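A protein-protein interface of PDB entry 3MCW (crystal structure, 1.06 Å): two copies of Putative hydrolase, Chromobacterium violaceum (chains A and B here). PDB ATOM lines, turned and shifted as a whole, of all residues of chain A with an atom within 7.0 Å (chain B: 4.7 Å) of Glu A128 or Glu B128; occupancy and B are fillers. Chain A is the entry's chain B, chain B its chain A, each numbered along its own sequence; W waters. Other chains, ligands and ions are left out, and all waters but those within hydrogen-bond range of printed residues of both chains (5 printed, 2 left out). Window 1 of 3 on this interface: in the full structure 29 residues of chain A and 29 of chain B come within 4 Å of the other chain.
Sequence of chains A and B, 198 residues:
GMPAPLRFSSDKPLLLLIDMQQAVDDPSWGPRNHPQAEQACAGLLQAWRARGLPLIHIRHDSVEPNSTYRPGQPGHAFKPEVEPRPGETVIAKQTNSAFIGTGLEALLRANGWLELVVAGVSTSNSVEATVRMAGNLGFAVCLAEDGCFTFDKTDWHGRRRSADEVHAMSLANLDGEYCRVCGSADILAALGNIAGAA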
ATOM      1  N   ILE A  18       2.881  27.985 -21.973  1.00  0.00           N
ATOM      2  CA  ILE A  18       4.140  28.407 -21.418  1.00  0.00           C
ATOM      3  C   ILE A  18       5.332  27.748 -22.098  1.00  0.00           C
ATOM      4  O   ILE A  18       5.557  26.546 -21.994  1.00  0.00           O
ATOM      5  CB  ILE A  18       4.189  28.150 -19.883  1.00  0.00           C
ATOM      6  CG1 ILE A  18       3.028  28.911 -19.198  1.00  0.00           C
ATOM      7  CG2 ILE A  18       5.552  28.519 -19.318  1.00  0.00           C
ATOM      8  CD1 ILE A  18       2.920  28.722 -17.731  1.00  0.00           C
ATOM      9  N   ASN A  96      11.664  32.650 -14.496  1.00  0.00           N
ATOM     10  CA  ASN A  96      10.776  31.476 -14.581  1.00  0.00           C
ATOM     11  C   ASN A  96       9.296  31.812 -14.574  1.00  0.00           C
ATOM     12  O   ASN A  96       8.524  31.288 -15.365  1.00  0.00           O
ATOM     13  CB  ASN A  96      11.103  30.492 -13.453  1.00  0.00           C
ATOM     14  CG  ASN A  96      12.544  30.119 -13.467  1.00  0.00           C
ATOM     15  OD1 ASN A  96      13.335  30.666 -12.708  1.00  0.00           O
ATOM     16  ND2 ASN A  96      12.927  29.259 -14.417  1.00  0.00           N
ATOM     17  N   SER A  97       8.856  32.654 -13.647  1.00  0.00           N
ATOM     18  CA  SER A  97       7.458  33.006 -13.573  1.00  0.00           C
ATOM     19  C   SER A  97       7.021  33.989 -14.664  1.00  0.00           C
ATOM     20  O   SER A  97       7.635  35.029 -14.840  1.00  0.00           O
ATOM     21  CB  SER A  97       7.139  33.607 -12.219  1.00  0.00           C
ATOM     22  OG  SER A  97       5.806  34.111 -12.266  1.00  0.00           O
ATOM     23  N   SER A 122       8.689  23.709 -18.441  1.00  0.00           N
ATOM     24  CA  SER A 122       8.581  22.377 -17.837  1.00  0.00           C
ATOM     25  C   SER A 122       7.624  22.404 -16.658  1.00  0.00           C
ATOM     26  O   SER A 122       7.493  23.413 -15.972  1.00  0.00           O
ATOM     27  CB  SER A 122       9.921  21.854 -17.392  1.00  0.00           C
ATOM     28  OG  SER A 122      10.259  22.339 -16.146  1.00  0.00           O
ATOM     29  N   THR A 123       6.980  21.263 -16.409  1.00  0.00           N
ATOM     30  CA  THR A 123       6.009  21.167 -15.309  1.00  0.00           C
ATOM     31  C   THR A 123       6.600  21.739 -14.017  1.00  0.00           C
ATOM     32  O   THR A 123       5.904  22.463 -13.307  1.00  0.00           O
ATOM     33  CB  THR A 123       5.624  19.706 -15.052  1.00  0.00           C
ATOM     34  OG1 THR A 123       5.358  19.097 -16.315  1.00  0.00           O
ATOM     35  CG2 THR A 123       4.418  19.585 -14.122  1.00  0.00           C
ATOM     36  N   SER A 124       7.845  21.347 -13.715  1.00  0.00           N
ATOM     37  CA  SER A 124       8.473  21.590 -12.437  1.00  0.00           C
ATOM     38  C   SER A 124       9.251  22.887 -12.344  1.00  0.00           C
ATOM     39  O   SER A 124       9.667  23.260 -11.238  1.00  0.00           O
ATOM     40  CB  SER A 124       9.362  20.387 -12.101  1.00  0.00           C
ATOM     41  OG  SER A 124      10.214  20.121 -13.210  1.00  0.00           O
ATOM     42  N   ASN A 125       9.496  23.542 -13.468  1.00  0.00           N
ATOM     43  CA  ASN A 125      10.294  24.770 -13.468  1.00  0.00           C
ATOM     44  C   ASN A 125       9.369  25.947 -13.780  1.00  0.00           C
ATOM     45  O   ASN A 125       8.692  26.413 -12.884  1.00  0.00           O
ATOM     46  CB  ASN A 125      11.576  24.619 -14.294  1.00  0.00           C
ATOM     47  CG  ASN A 125      12.530  25.723 -13.993  1.00  0.00           C
ATOM     48  OD1 ASN A 125      12.456  26.378 -12.940  1.00  0.00           O
ATOM     49  ND2 ASN A 125      13.499  25.905 -14.850  1.00  0.00           N
ATOM     50  N   SER A 126       9.309  26.398 -15.019  1.00  0.00           N
ATOM     51  CA  SER A 126       8.565  27.603 -15.310  1.00  0.00           C
ATOM     52  C   SER A 126       7.062  27.434 -15.189  1.00  0.00           C
ATOM     53  O   SER A 126       6.372  28.385 -14.828  1.00  0.00           O
ATOM     54  CB  SER A 126       8.939  28.178 -16.672  1.00  0.00           C
ATOM     55  OG  SER A 126      10.259  28.703 -16.654  1.00  0.00           O
ATOM     56  N   VAL A 127       6.521  26.249 -15.495  1.00  0.00           N
ATOM     57  CA  VAL A 127       5.099  26.050 -15.296  1.00  0.00           C
ATOM     58  C   VAL A 127       4.765  26.165 -13.794  1.00  0.00           C
ATOM     59  O   VAL A 127       3.906  26.944 -13.407  1.00  0.00           O
ATOM     60  CB  VAL A 127       4.580  24.722 -15.894  1.00  0.00           C
ATOM     61  CG1 VAL A 127       3.122  24.479 -15.515  1.00  0.00           C
ATOM     62  CG2 VAL A 127       4.750  24.727 -17.426  1.00  0.00           C
ATOM     63  N   GLU A 128       5.461  25.409 -12.970  1.00  0.00           N
ATOM     64  CA  GLU A 128       5.229  25.453 -11.535  1.00  0.00           C
ATOM     65  C   GLU A 128       5.439  26.867 -10.980  1.00  0.00           C
ATOM     66  O   GLU A 128       4.639  27.326 -10.158  1.00  0.00           O
ATOM     67  CB  GLU A 128       6.097  24.453 -10.819  1.00  0.00           C
ATOM     68  CG  GLU A 128       5.967  24.485  -9.340  1.00  0.00           C
ATOM     69  CD  GLU A 128       6.442  23.242  -8.624  1.00  0.00           C
ATOM     70  OE1 GLU A 128       6.857  22.252  -9.228  1.00  0.00           O
ATOM     71  OE2 GLU A 128       6.383  23.305  -7.398  1.00  0.00           O
ATOM     72  N   ALA A 129       6.483  27.553 -11.398  1.00  0.00           N
ATOM     73  CA  ALA A 129       6.737  28.909 -10.882  1.00  0.00           C
ATOM     74  C   ALA A 129       5.565  29.842 -11.196  1.00  0.00           C
ATOM     75  O   ALA A 129       5.103  30.629 -10.373  1.00  0.00           O
ATOM     76  CB  ALA A 129       8.024  29.484 -11.458  1.00  0.00           C
ATOM     77  N   THR A 130       5.063  29.739 -12.421  1.00  0.00           N
ATOM     78  CA  THR A 130       3.953  30.529 -12.879  1.00  0.00           C
ATOM     79  C   THR A 130       2.670  30.196 -12.138  1.00  0.00           C
ATOM     80  O   THR A 130       1.916  31.084 -11.751  1.00  0.00           O
ATOM     81  CB  THR A 130       3.792  30.407 -14.410  1.00  0.00           C
ATOM     82  OG1 THR A 130       4.983  30.876 -15.052  1.00  0.00           O
ATOM     83  CG2 THR A 130       2.601  31.195 -14.897  1.00  0.00           C
ATOM     84  N   VAL A 131       2.374  28.897 -12.007  1.00  0.00           N
ATOM     85  CA  VAL A 131       1.148  28.475 -11.359  1.00  0.00           C
ATOM     86  C   VAL A 131       1.133  28.801  -9.872  1.00  0.00           C
ATOM     87  O   VAL A 131       0.112  29.220  -9.344  1.00  0.00           O
ATOM     88  CB  VAL A 131       0.869  26.973 -11.607  1.00  0.00           C
ATOM     89  CG1 VAL A 131      -0.314  26.501 -10.803  1.00  0.00           C
ATOM     90  CG2 VAL A 131       0.666  26.704 -13.102  1.00  0.00           C
ATOM     91  N   ARG A 132       2.255  28.604  -9.193  1.00  0.00           N
ATOM     92  CA  ARG A 132       2.280  28.964  -7.754  1.00  0.00           C
ATOM     93  C   ARG A 132       1.932  30.438  -7.574  1.00  0.00           C
ATOM     94  O   ARG A 132       1.157  30.791  -6.699  1.00  0.00           O
ATOM     95  CB  ARG A 132       3.605  28.635  -7.094  1.00  0.00           C
ATOM     96  CG  ARG A 132       3.859  27.156  -6.868  1.00  0.00           C
ATOM     97  CD  ARG A 132       5.096  26.920  -6.043  1.00  0.00           C
ATOM     98  NE  ARG A 132       5.448  25.515  -5.843  1.00  0.00           N
ATOM     99  CZ  ARG A 132       5.664  24.942  -4.663  1.00  0.00           C
ATOM    100  NH1 ARG A 132       5.429  25.552  -3.507  1.00  0.00           N
ATOM    101  NH2 ARG A 132       6.181  23.726  -4.632  1.00  0.00           N
ATOM    102  N   MET A 133       2.548  31.300  -8.383  1.00  0.00           N
ATOM    103  CA  MET A 133       2.227  32.716  -8.267  1.00  0.00           C
ATOM    104  C   MET A 133       0.795  33.012  -8.671  1.00  0.00           C
ATOM    105  O   MET A 133       0.114  33.786  -8.012  1.00  0.00           O
ATOM    106  CB  MET A 133       3.159  33.591  -9.046  1.00  0.00           C
ATOM    107  CG  MET A 133       4.466  33.786  -8.373  1.00  0.00           C
ATOM    108  SD  MET A 133       5.583  35.157  -9.204  1.00  0.00           S
ATOM    109  CE  MET A 133       4.396  36.706  -8.983  1.00  0.00           C
ATOM    110  N   ALA A 134       0.306  32.418  -9.766  1.00  0.00           N
ATOM    111  CA  ALA A 134      -1.069  32.678 -10.202  1.00  0.00           C
ATOM    112  C   ALA A 134      -2.033  32.348  -9.104  1.00  0.00           C
ATOM    113  O   ALA A 134      -2.958  33.107  -8.830  1.00  0.00           O
ATOM    114  CB  ALA A 134      -1.391  31.873 -11.470  1.00  0.00           C
ATOM    115  N   LEU A 143      -4.727  23.449 -14.349  1.00  0.00           N
ATOM    116  CA  LEU A 143      -3.470  23.037 -14.948  1.00  0.00           C
ATOM    117  C   LEU A 143      -3.759  21.792 -15.769  1.00  0.00           C
ATOM    118  O   LEU A 143      -4.134  20.747 -15.241  1.00  0.00           O
ATOM    119  CB  LEU A 143      -2.446  22.737 -13.863  1.00  0.00           C
ATOM    120  CG  LEU A 143      -1.073  22.282 -14.355  1.00  0.00           C
ATOM    121  CD1 LEU A 143      -0.452  23.307 -15.279  1.00  0.00           C
ATOM    122  CD2 LEU A 143      -0.150  22.083 -13.151  1.00  0.00           C
ATOM    123  N   VAL A 166       9.259  13.363 -11.429  1.00  0.00           N
ATOM    124  CA  VAL A 166       9.414  14.810 -11.237  1.00  0.00           C
ATOM    125  C   VAL A 166       8.061  15.482 -11.467  1.00  0.00           C
ATOM    126  O   VAL A 166       7.612  16.334 -10.674  1.00  0.00           O
ATOM    127  CB  VAL A 166      10.498  15.380 -12.132  1.00  0.00           C
ATOM    128  CG1 VAL A 166      10.569  16.878 -12.031  1.00  0.00           C
ATOM    129  CG2 VAL A 166      11.849  14.767 -11.806  1.00  0.00           C
ATOM    130  N   HIS A 167       7.420  15.121 -12.579  1.00  0.00           N
ATOM    131  CA  HIS A 167       6.086  15.634 -12.915  1.00  0.00           C
ATOM    132  C   HIS A 167       5.084  15.346 -11.813  1.00  0.00           C
ATOM    133  O   HIS A 167       4.336  16.211 -11.384  1.00  0.00           O
ATOM    134  CB  HIS A 167       5.696  14.978 -14.250  1.00  0.00           C
ATOM    135  CG  HIS A 167       4.410  15.435 -14.843  1.00  0.00           C
ATOM    136  ND1 HIS A 167       4.308  16.495 -15.735  1.00  0.00           N
ATOM    137  CD2 HIS A 167       3.171  14.904 -14.715  1.00  0.00           C
ATOM    138  CE1 HIS A 167       3.040  16.578 -16.117  1.00  0.00           C
ATOM    139  NE2 HIS A 167       2.318  15.632 -15.517  1.00  0.00           N
ATOM    140  N   MET A 169       5.518  14.622  -8.667  1.00  0.00           N
ATOM    141  CA  MET A 169       5.762  15.317  -7.395  1.00  0.00           C
ATOM    142  C   MET A 169       5.334  16.796  -7.523  1.00  0.00           C
ATOM    143  O   MET A 169       4.708  17.334  -6.611  1.00  0.00           O
ATOM    144  CB  MET A 169       7.226  15.109  -6.927  1.00  0.00           C
ATOM    145  CG  MET A 169       7.505  13.672  -6.431  1.00  0.00           C
ATOM    146  SD  MET A 169       9.344  13.285  -5.776  1.00  0.00           S
ATOM    147  CE  MET A 169       9.049  13.976  -4.057  1.00  0.00           C
ATOM    148  N   SER A 170       5.640  17.438  -8.658  1.00  0.00           N
ATOM    149  CA  SER A 170       5.190  18.813  -8.825  1.00  0.00           C
ATOM    150  C   SER A 170       3.679  18.910  -8.841  1.00  0.00           C
ATOM    151  O   SER A 170       3.114  19.795  -8.190  1.00  0.00           O
ATOM    152  CB  SER A 170       5.752  19.463 -10.066  1.00  0.00           C
ATOM    153  OG  SER A 170       7.118  19.761  -9.906  1.00  0.00           O
ATOM    154  N   LEU A 171       2.976  18.015  -9.529  1.00  0.00           N
ATOM    155  CA  LEU A 171       1.519  18.070  -9.543  1.00  0.00           C
ATOM    156  C   LEU A 171       0.957  17.911  -8.126  1.00  0.00           C
ATOM    157  O   LEU A 171      -0.022  18.553  -7.771  1.00  0.00           O
ATOM    158  CB  LEU A 171       0.914  17.008 -10.472  1.00  0.00           C
ATOM    159  CG  LEU A 171       1.178  17.157 -11.970  1.00  0.00           C
ATOM    160  CD1 LEU A 171       0.435  16.039 -12.680  1.00  0.00           C
ATOM    161  CD2 LEU A 171       0.832  18.529 -12.507  1.00  0.00           C
ATOM    162  N   ASN A 173       2.352  18.784  -5.342  1.00  0.00           N
ATOM    163  CA  ASN A 173       2.580  20.023  -4.622  1.00  0.00           C
ATOM    164  C   ASN A 173       1.643  21.149  -5.081  1.00  0.00           C
ATOM    165  O   ASN A 173       1.322  22.055  -4.304  1.00  0.00           O
ATOM    166  CB  ASN A 173       4.042  20.444  -4.752  1.00  0.00           C
ATOM    167  CG  ASN A 173       4.992  19.574  -3.922  1.00  0.00           C
ATOM    168  OD1 ASN A 173       4.558  18.869  -3.009  1.00  0.00           O
ATOM    169  ND2 ASN A 173       6.261  19.568  -4.302  1.00  0.00           N
ATOM    170  N   LEU A 174       1.210  21.099  -6.336  1.00  0.00           N
ATOM    171  CA  LEU A 174       0.384  22.153  -6.907  1.00  0.00           C
ATOM    172  C   LEU A 174      -1.105  21.977  -6.668  1.00  0.00           C
ATOM    173  O   LEU A 174      -1.829  22.959  -6.453  1.00  0.00           O
ATOM    174  CB  LEU A 174       0.655  22.249  -8.421  1.00  0.00           C
ATOM    175  CG  LEU A 174       2.012  22.811  -8.795  1.00  0.00           C
ATOM    176  CD1 LEU A 174       2.258  22.657 -10.292  1.00  0.00           C
ATOM    177  CD2 LEU A 174       2.034  24.316  -8.470  1.00  0.00           C
ATOM    178  N   TYR A 178      -2.592  25.431  -5.033  1.00  0.00           N
ATOM    179  CA  TYR A 178      -2.341  26.472  -6.032  1.00  0.00           C
ATOM    180  C   TYR A 178      -3.256  26.438  -7.252  1.00  0.00           C
ATOM    181  O   TYR A 178      -3.370  27.443  -7.954  1.00  0.00           O
ATOM    182  CB  TYR A 178      -0.900  26.416  -6.500  1.00  0.00           C
ATOM    183  CG  TYR A 178       0.113  26.575  -5.409  1.00  0.00           C
ATOM    184  CD1 TYR A 178       0.566  27.822  -4.996  1.00  0.00           C
ATOM    185  CD2 TYR A 178       0.661  25.462  -4.775  1.00  0.00           C
ATOM    186  CE1 TYR A 178       1.553  27.971  -4.009  1.00  0.00           C
ATOM    187  CE2 TYR A 178       1.614  25.585  -3.758  1.00  0.00           C
ATOM    188  CZ  TYR A 178       2.058  26.844  -3.387  1.00  0.00           C
ATOM    189  OH  TYR A 178       3.031  26.996  -2.402  1.00  0.00           O
ATOM    190  N   SER B 122       6.798  24.834   5.254  1.00  0.00           N
ATOM    191  CA  SER B 122       7.430  23.589   4.820  1.00  0.00           C
ATOM    192  C   SER B 122       8.330  23.834   3.624  1.00  0.00           C
ATOM    193  O   SER B 122       8.092  24.725   2.788  1.00  0.00           O
ATOM    194  CB  SER B 122       6.416  22.539   4.467  1.00  0.00           C
ATOM    195  OG  SER B 122       5.923  22.730   3.183  1.00  0.00           O
ATOM    196  N   THR B 123       9.344  22.993   3.499  1.00  0.00           N
ATOM    197  CA  THR B 123      10.315  23.149   2.410  1.00  0.00           C
ATOM    198  C   THR B 123       9.620  23.299   1.073  1.00  0.00           C
ATOM    199  O   THR B 123      10.008  24.136   0.256  1.00  0.00           O
ATOM    200  CB  THR B 123      11.245  21.929   2.337  1.00  0.00           C
ATOM    201  OG1 THR B 123      11.695  21.621   3.656  1.00  0.00           O
ATOM    202  CG2 THR B 123      12.427  22.198   1.408  1.00  0.00           C
ATOM    203  N   SER B 124       8.629  22.443   0.820  1.00  0.00           N
ATOM    204  CA  SER B 124       8.023  22.280  -0.475  1.00  0.00           C
ATOM    205  C   SER B 124       6.775  23.135  -0.697  1.00  0.00           C
ATOM    206  O   SER B 124       6.275  23.180  -1.808  1.00  0.00           O
ATOM    207  CB  SER B 124       7.683  20.800  -0.649  1.00  0.00           C
ATOM    208  OG  SER B 124       6.949  20.328   0.479  1.00  0.00           O
ATOM    209  N   ASN B 125       6.269  23.798   0.352  1.00  0.00           N
ATOM    210  CA  ASN B 125       5.074  24.607   0.246  1.00  0.00           C
ATOM    211  C   ASN B 125       5.446  26.087   0.423  1.00  0.00           C
ATOM    212  O   ASN B 125       5.929  26.694  -0.538  1.00  0.00           O
ATOM    213  CB  ASN B 125       3.940  24.069   1.110  1.00  0.00           C
ATOM    214  CG  ASN B 125       2.615  24.690   0.724  1.00  0.00           C
ATOM    215  OD1 ASN B 125       2.479  25.275  -0.356  1.00  0.00           O
ATOM    216  ND2 ASN B 125       1.633  24.518   1.549  1.00  0.00           N
ATOM    217  N   SER B 126       5.270  26.674   1.604  1.00  0.00           N
ATOM    218  CA  SER B 126       5.525  28.099   1.744  1.00  0.00           C
ATOM    219  C   SER B 126       6.977  28.499   1.582  1.00  0.00           C
ATOM    220  O   SER B 126       7.260  29.600   1.093  1.00  0.00           O
ATOM    221  CB  SER B 126       4.957  28.613   3.059  1.00  0.00           C
ATOM    222  OG  SER B 126       3.536  28.624   3.030  1.00  0.00           O
ATOM    223  N   VAL B 127       7.919  27.656   2.017  1.00  0.00           N
ATOM    224  CA  VAL B 127       9.330  27.992   1.807  1.00  0.00           C
ATOM    225  C   VAL B 127       9.631  28.032   0.293  1.00  0.00           C
ATOM    226  O   VAL B 127      10.126  29.023  -0.210  1.00  0.00           O
ATOM    227  CB  VAL B 127      10.281  27.032   2.524  1.00  0.00           C
ATOM    228  CG1 VAL B 127      11.694  27.300   2.157  1.00  0.00           C
ATOM    229  CG2 VAL B 127      10.095  27.139   4.064  1.00  0.00           C
ATOM    230  N   GLU B 128       9.277  26.977  -0.430  1.00  0.00           N
ATOM    231  CA  GLU B 128       9.514  26.933  -1.862  1.00  0.00           C
ATOM    232  C   GLU B 128       8.788  28.080  -2.584  1.00  0.00           C
ATOM    233  O   GLU B 128       9.396  28.685  -3.478  1.00  0.00           O
ATOM    234  CB  GLU B 128       9.107  25.584  -2.416  1.00  0.00           C
ATOM    235  CG  GLU B 128       9.297  25.472  -3.914  1.00  0.00           C
ATOM    236  CD  GLU B 128       9.407  24.061  -4.442  1.00  0.00           C
ATOM    237  OE1 GLU B 128       9.332  23.090  -3.668  1.00  0.00           O
ATOM    238  OE2 GLU B 128       9.555  24.002  -5.673  1.00  0.00           O
ATOM    239  N   ALA B 129       7.551  28.363  -2.235  1.00  0.00           N
ATOM    240  CA  ALA B 129       6.828  29.452  -2.920  1.00  0.00           C
ATOM    241  C   ALA B 129       7.553  30.776  -2.736  1.00  0.00           C
ATOM    242  O   ALA B 129       7.716  31.580  -3.664  1.00  0.00           O
ATOM    243  CB  ALA B 129       5.401  29.565  -2.383  1.00  0.00           C
ATOM    244  N   THR B 130       8.024  31.016  -1.506  1.00  0.00           N
ATOM    245  CA  THR B 130       8.723  32.241  -1.180  1.00  0.00           C
ATOM    246  C   THR B 130      10.064  32.331  -1.881  1.00  0.00           C
ATOM    247  O   THR B 130      10.429  33.384  -2.407  1.00  0.00           O
ATOM    248  CB  THR B 130       8.852  32.374   0.346  1.00  0.00           C
ATOM    249  OG1 THR B 130       7.564  32.427   0.960  1.00  0.00           O
ATOM    250  CG2 THR B 130       9.599  33.620   0.730  1.00  0.00           C
ATOM    251  N   VAL B 131      10.829  31.241  -1.867  1.00  0.00           N
ATOM    252  CA  VAL B 131      12.146  31.241  -2.479  1.00  0.00           C
ATOM    253  C   VAL B 131      12.074  31.376  -3.995  1.00  0.00           C
ATOM    254  O   VAL B 131      12.868  32.088  -4.592  1.00  0.00           O
ATOM    255  CB  VAL B 131      12.975  30.002  -2.053  1.00  0.00           C
ATOM    256  CG1 VAL B 131      14.268  29.922  -2.812  1.00  0.00           C
ATOM    257  CG2 VAL B 131      13.229  30.037  -0.556  1.00  0.00           C
ATOM    258  N   ARG B 132      11.133  30.682  -4.639  1.00  0.00           N
ATOM    259  CA  ARG B 132      11.019  30.807  -6.097  1.00  0.00           C
ATOM    260  C   ARG B 132      10.754  32.266  -6.453  1.00  0.00           C
ATOM    261  O   ARG B 132      11.376  32.789  -7.389  1.00  0.00           O
ATOM    262  CB  ARG B 132       9.956  29.897  -6.685  1.00  0.00           C
ATOM    263  CG  ARG B 132      10.326  28.432  -6.727  1.00  0.00           C
ATOM    264  CD  ARG B 132       9.287  27.614  -7.480  1.00  0.00           C
ATOM    265  NE  ARG B 132       9.535  26.178  -7.518  1.00  0.00           N
ATOM    266  CZ  ARG B 132       9.581  25.443  -8.631  1.00  0.00           C
ATOM    267  NH1 ARG B 132       9.527  25.958  -9.834  1.00  0.00           N
ATOM    268  NH2 ARG B 132       9.590  24.123  -8.507  1.00  0.00           N
ATOM    269  N   SER B 170      12.432  19.125  -3.776  1.00  0.00           N
ATOM    270  CA  SER B 170      12.324  20.591  -3.764  1.00  0.00           C
ATOM    271  C   SER B 170      13.668  21.271  -3.751  1.00  0.00           C
ATOM    272  O   SER B 170      13.886  22.224  -4.492  1.00  0.00           O
ATOM    273  CB  SER B 170      11.495  21.079  -2.595  1.00  0.00           C
ATOM    274  OG  SER B 170      10.131  20.789  -2.761  1.00  0.00           O
ATOM    275  N   ASN B 173      15.081  21.249  -7.257  1.00  0.00           N
ATOM    276  CA  ASN B 173      14.399  22.231  -8.116  1.00  0.00           C
ATOM    277  C   ASN B 173      14.782  23.665  -7.784  1.00  0.00           C
ATOM    278  O   ASN B 173      14.793  24.520  -8.667  1.00  0.00           O
ATOM    279  CB  ASN B 173      12.881  22.047  -8.041  1.00  0.00           C
ATOM    280  CG  ASN B 173      12.372  20.790  -8.807  1.00  0.00           C
ATOM    281  OD1 ASN B 173      13.070  20.249  -9.683  1.00  0.00           O
ATOM    282  ND2 ASN B 173      11.209  20.327  -8.434  1.00  0.00           N
ATOM    283  N   LEU B 174      15.093  23.929  -6.524  1.00  0.00           N
ATOM    284  CA  LEU B 174      15.424  25.268  -6.070  1.00  0.00           C
ATOM    285  C   LEU B 174      16.874  25.662  -6.325  1.00  0.00           C
ATOM    286  O   LEU B 174      17.152  26.820  -6.655  1.00  0.00           O
ATOM    287  CB  LEU B 174      15.087  25.414  -4.586  1.00  0.00           C
ATOM    288  CG  LEU B 174      13.610  25.447  -4.250  1.00  0.00           C
ATOM    289  CD1 LEU B 174      13.369  25.356  -2.756  1.00  0.00           C
ATOM    290  CD2 LEU B 174      12.970  26.751  -4.797  1.00  0.00           C
HETATM  291  O   HOH W   1      12.693  20.031 -12.383  1.00  0.00           O
HETATM  292  O   HOH W   2       8.400  33.208  -9.119  1.00  0.00           O
HETATM  293  O   HOH W   3       4.742  19.121  -0.348  1.00  0.00           O
HETATM  294  O   HOH W   4       9.177  18.151  -8.941  1.00  0.00           O
HETATM  295  O   HOH W   5       8.935  18.471  -3.586  1.00  0.00           O
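The side-chain amide oxygen of Asn B125 sits at hydrogen-bond distance from the side-chain hydroxyl of Tyr A178 (2.7 Å). NH2 of Arg A132 sits at hydrogen-bond distance from O of Ser B124 (2.9 Å). The guanidinium group of Arg B132 sits at hydrogen-bond distance from the backbone carbonyl oxygen of Asn A125, 3.2 Å away. The backbone carbonyl oxygen (O) of Ser A124 lies within hydrogen-bond range of the guanidinium group (NH2) of Arg B132 (2.9 Å). O of Asn B125 lies within hydrogen-bond range of NH1 of Arg A132, 3.2 Å away. The guanidinium group of Arg B132 is in salt-bridge range of the side-chain carboxylate of Glu A128 (3.4 Å). The side-chain carboxylate (OE1) of Glu B128 lies within salt-bridge range of the guanidinium group (NH2) of Arg A132 (3.4 Å).
The side-chain carboxylate (OE1) of Glu A128 sits at hydrogen-bond distance from the side-chain hydroxyl (OG) of Ser A170 (2.6 Å). The side-chain carboxylate (OE1) of Glu B128 lies within hydrogen-bond range of the side-chain hydroxyl (OG) of Ser B170, at 2.6 Å. The guanidinium group (NH2) of Arg A132 is in salt-bridge range of the side-chain carboxylate (OE2) of Glu A128 (2.8 Å). The side-chain amide nitrogen (ND2) of Asn A96 sits at hydrogen-bond distance from the side-chain amide oxygen (OD1) of Asn A125 (3.3 Å). The side-chain hydroxyl (OG) of Ser B122 sits at hydrogen-bond distance from the backbone NH (N) of Asn B125 (3.0 Å).
Among the printed residues, pairs that only touch across the chains: Glu A128 with Glu B128 (3.7 Å), Ala A129 with Arg B132 (3.8 Å), Arg A132 with Ala B129 (3.7 Å) and Tyr A178 with Ala B129 (3.5 Å).
Glu A128 touches just these residues of chain B: Glu B128 and Arg B132. Of the printed residues of chain A, Glu B128 touches Glu A128 and Arg A132. Of the printed residues of chain A, Asn B125 touches Arg A132 and Tyr A178. Of the printed residues of chain B, Ser A124 touches Arg B132. Leu A143 touches none of the printed residues of chain B. Val B127 touches none of the printed residues of chain A. The nearest printed residue of chain A that does not touch Arg B132 is Arg A132 (4.5 Å).
Of the 14 printed residues of chain B, 5 touch a printed residue of chain A. Printed residues of chain B that touch a printed residue of chain A: Ser B124, Asn B125, Glu B128, Ala B129 and Arg B132. Hydrophobic or aromatic side chains of chain B that line the printed part of chain A: Ala B129. Hydrophobic or aromatic side chains of chain A that line the printed part of chain B: Tyr A178. Among the printed residues, Asp or Glu carboxylates within 4 Å of a Lys or Arg side-chain nitrogen of the other chain: Glu A128 with Arg B132 (3.4 Å) and Arg A132 with Glu B128 (3.4 Å).
Asn A125 touches Arg B132, and with the chains exchanged Arg A132 touches Asn B125. Glu B128 touches its own counterpart, Glu A128. Glu A128 touches Arg B132, and with the chains exchanged Arg A132 touches Glu B128. Ala A129 touches Arg B132, and with the chains exchanged Arg A132 touches Ala B129. Positions printed for both chains: 122, 123, 124, 125, 126, 127, 128, 129, 130, 131, 132, 170, 173 and 174.
Water W1 lies within hydrogen-bond range of OG of Ser A124 (2.6 Å) and OD1 of Asn B173 (2.7 Å). Water W3 bridges OG of Ser B124 (2.6 Å) and OD1 of Asn A173 (2.7 Å). Water W5 lies within hydrogen-bond range of OG of Ser B170 (2.7 Å) and ND2 of Asn A173 (3.0 Å). Water W4 lies within hydrogen-bond range of the side-chain hydroxyl of Ser A170 (2.8 Å), the backbone carbonyl oxygen of Val A166 (3.0 Å) and the side-chain amide nitrogen of Asn B173 (3.0 Å). Water W2 bridges SD of Met A133 (3.4 Å) and O of Arg B132 (3.5 Å).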
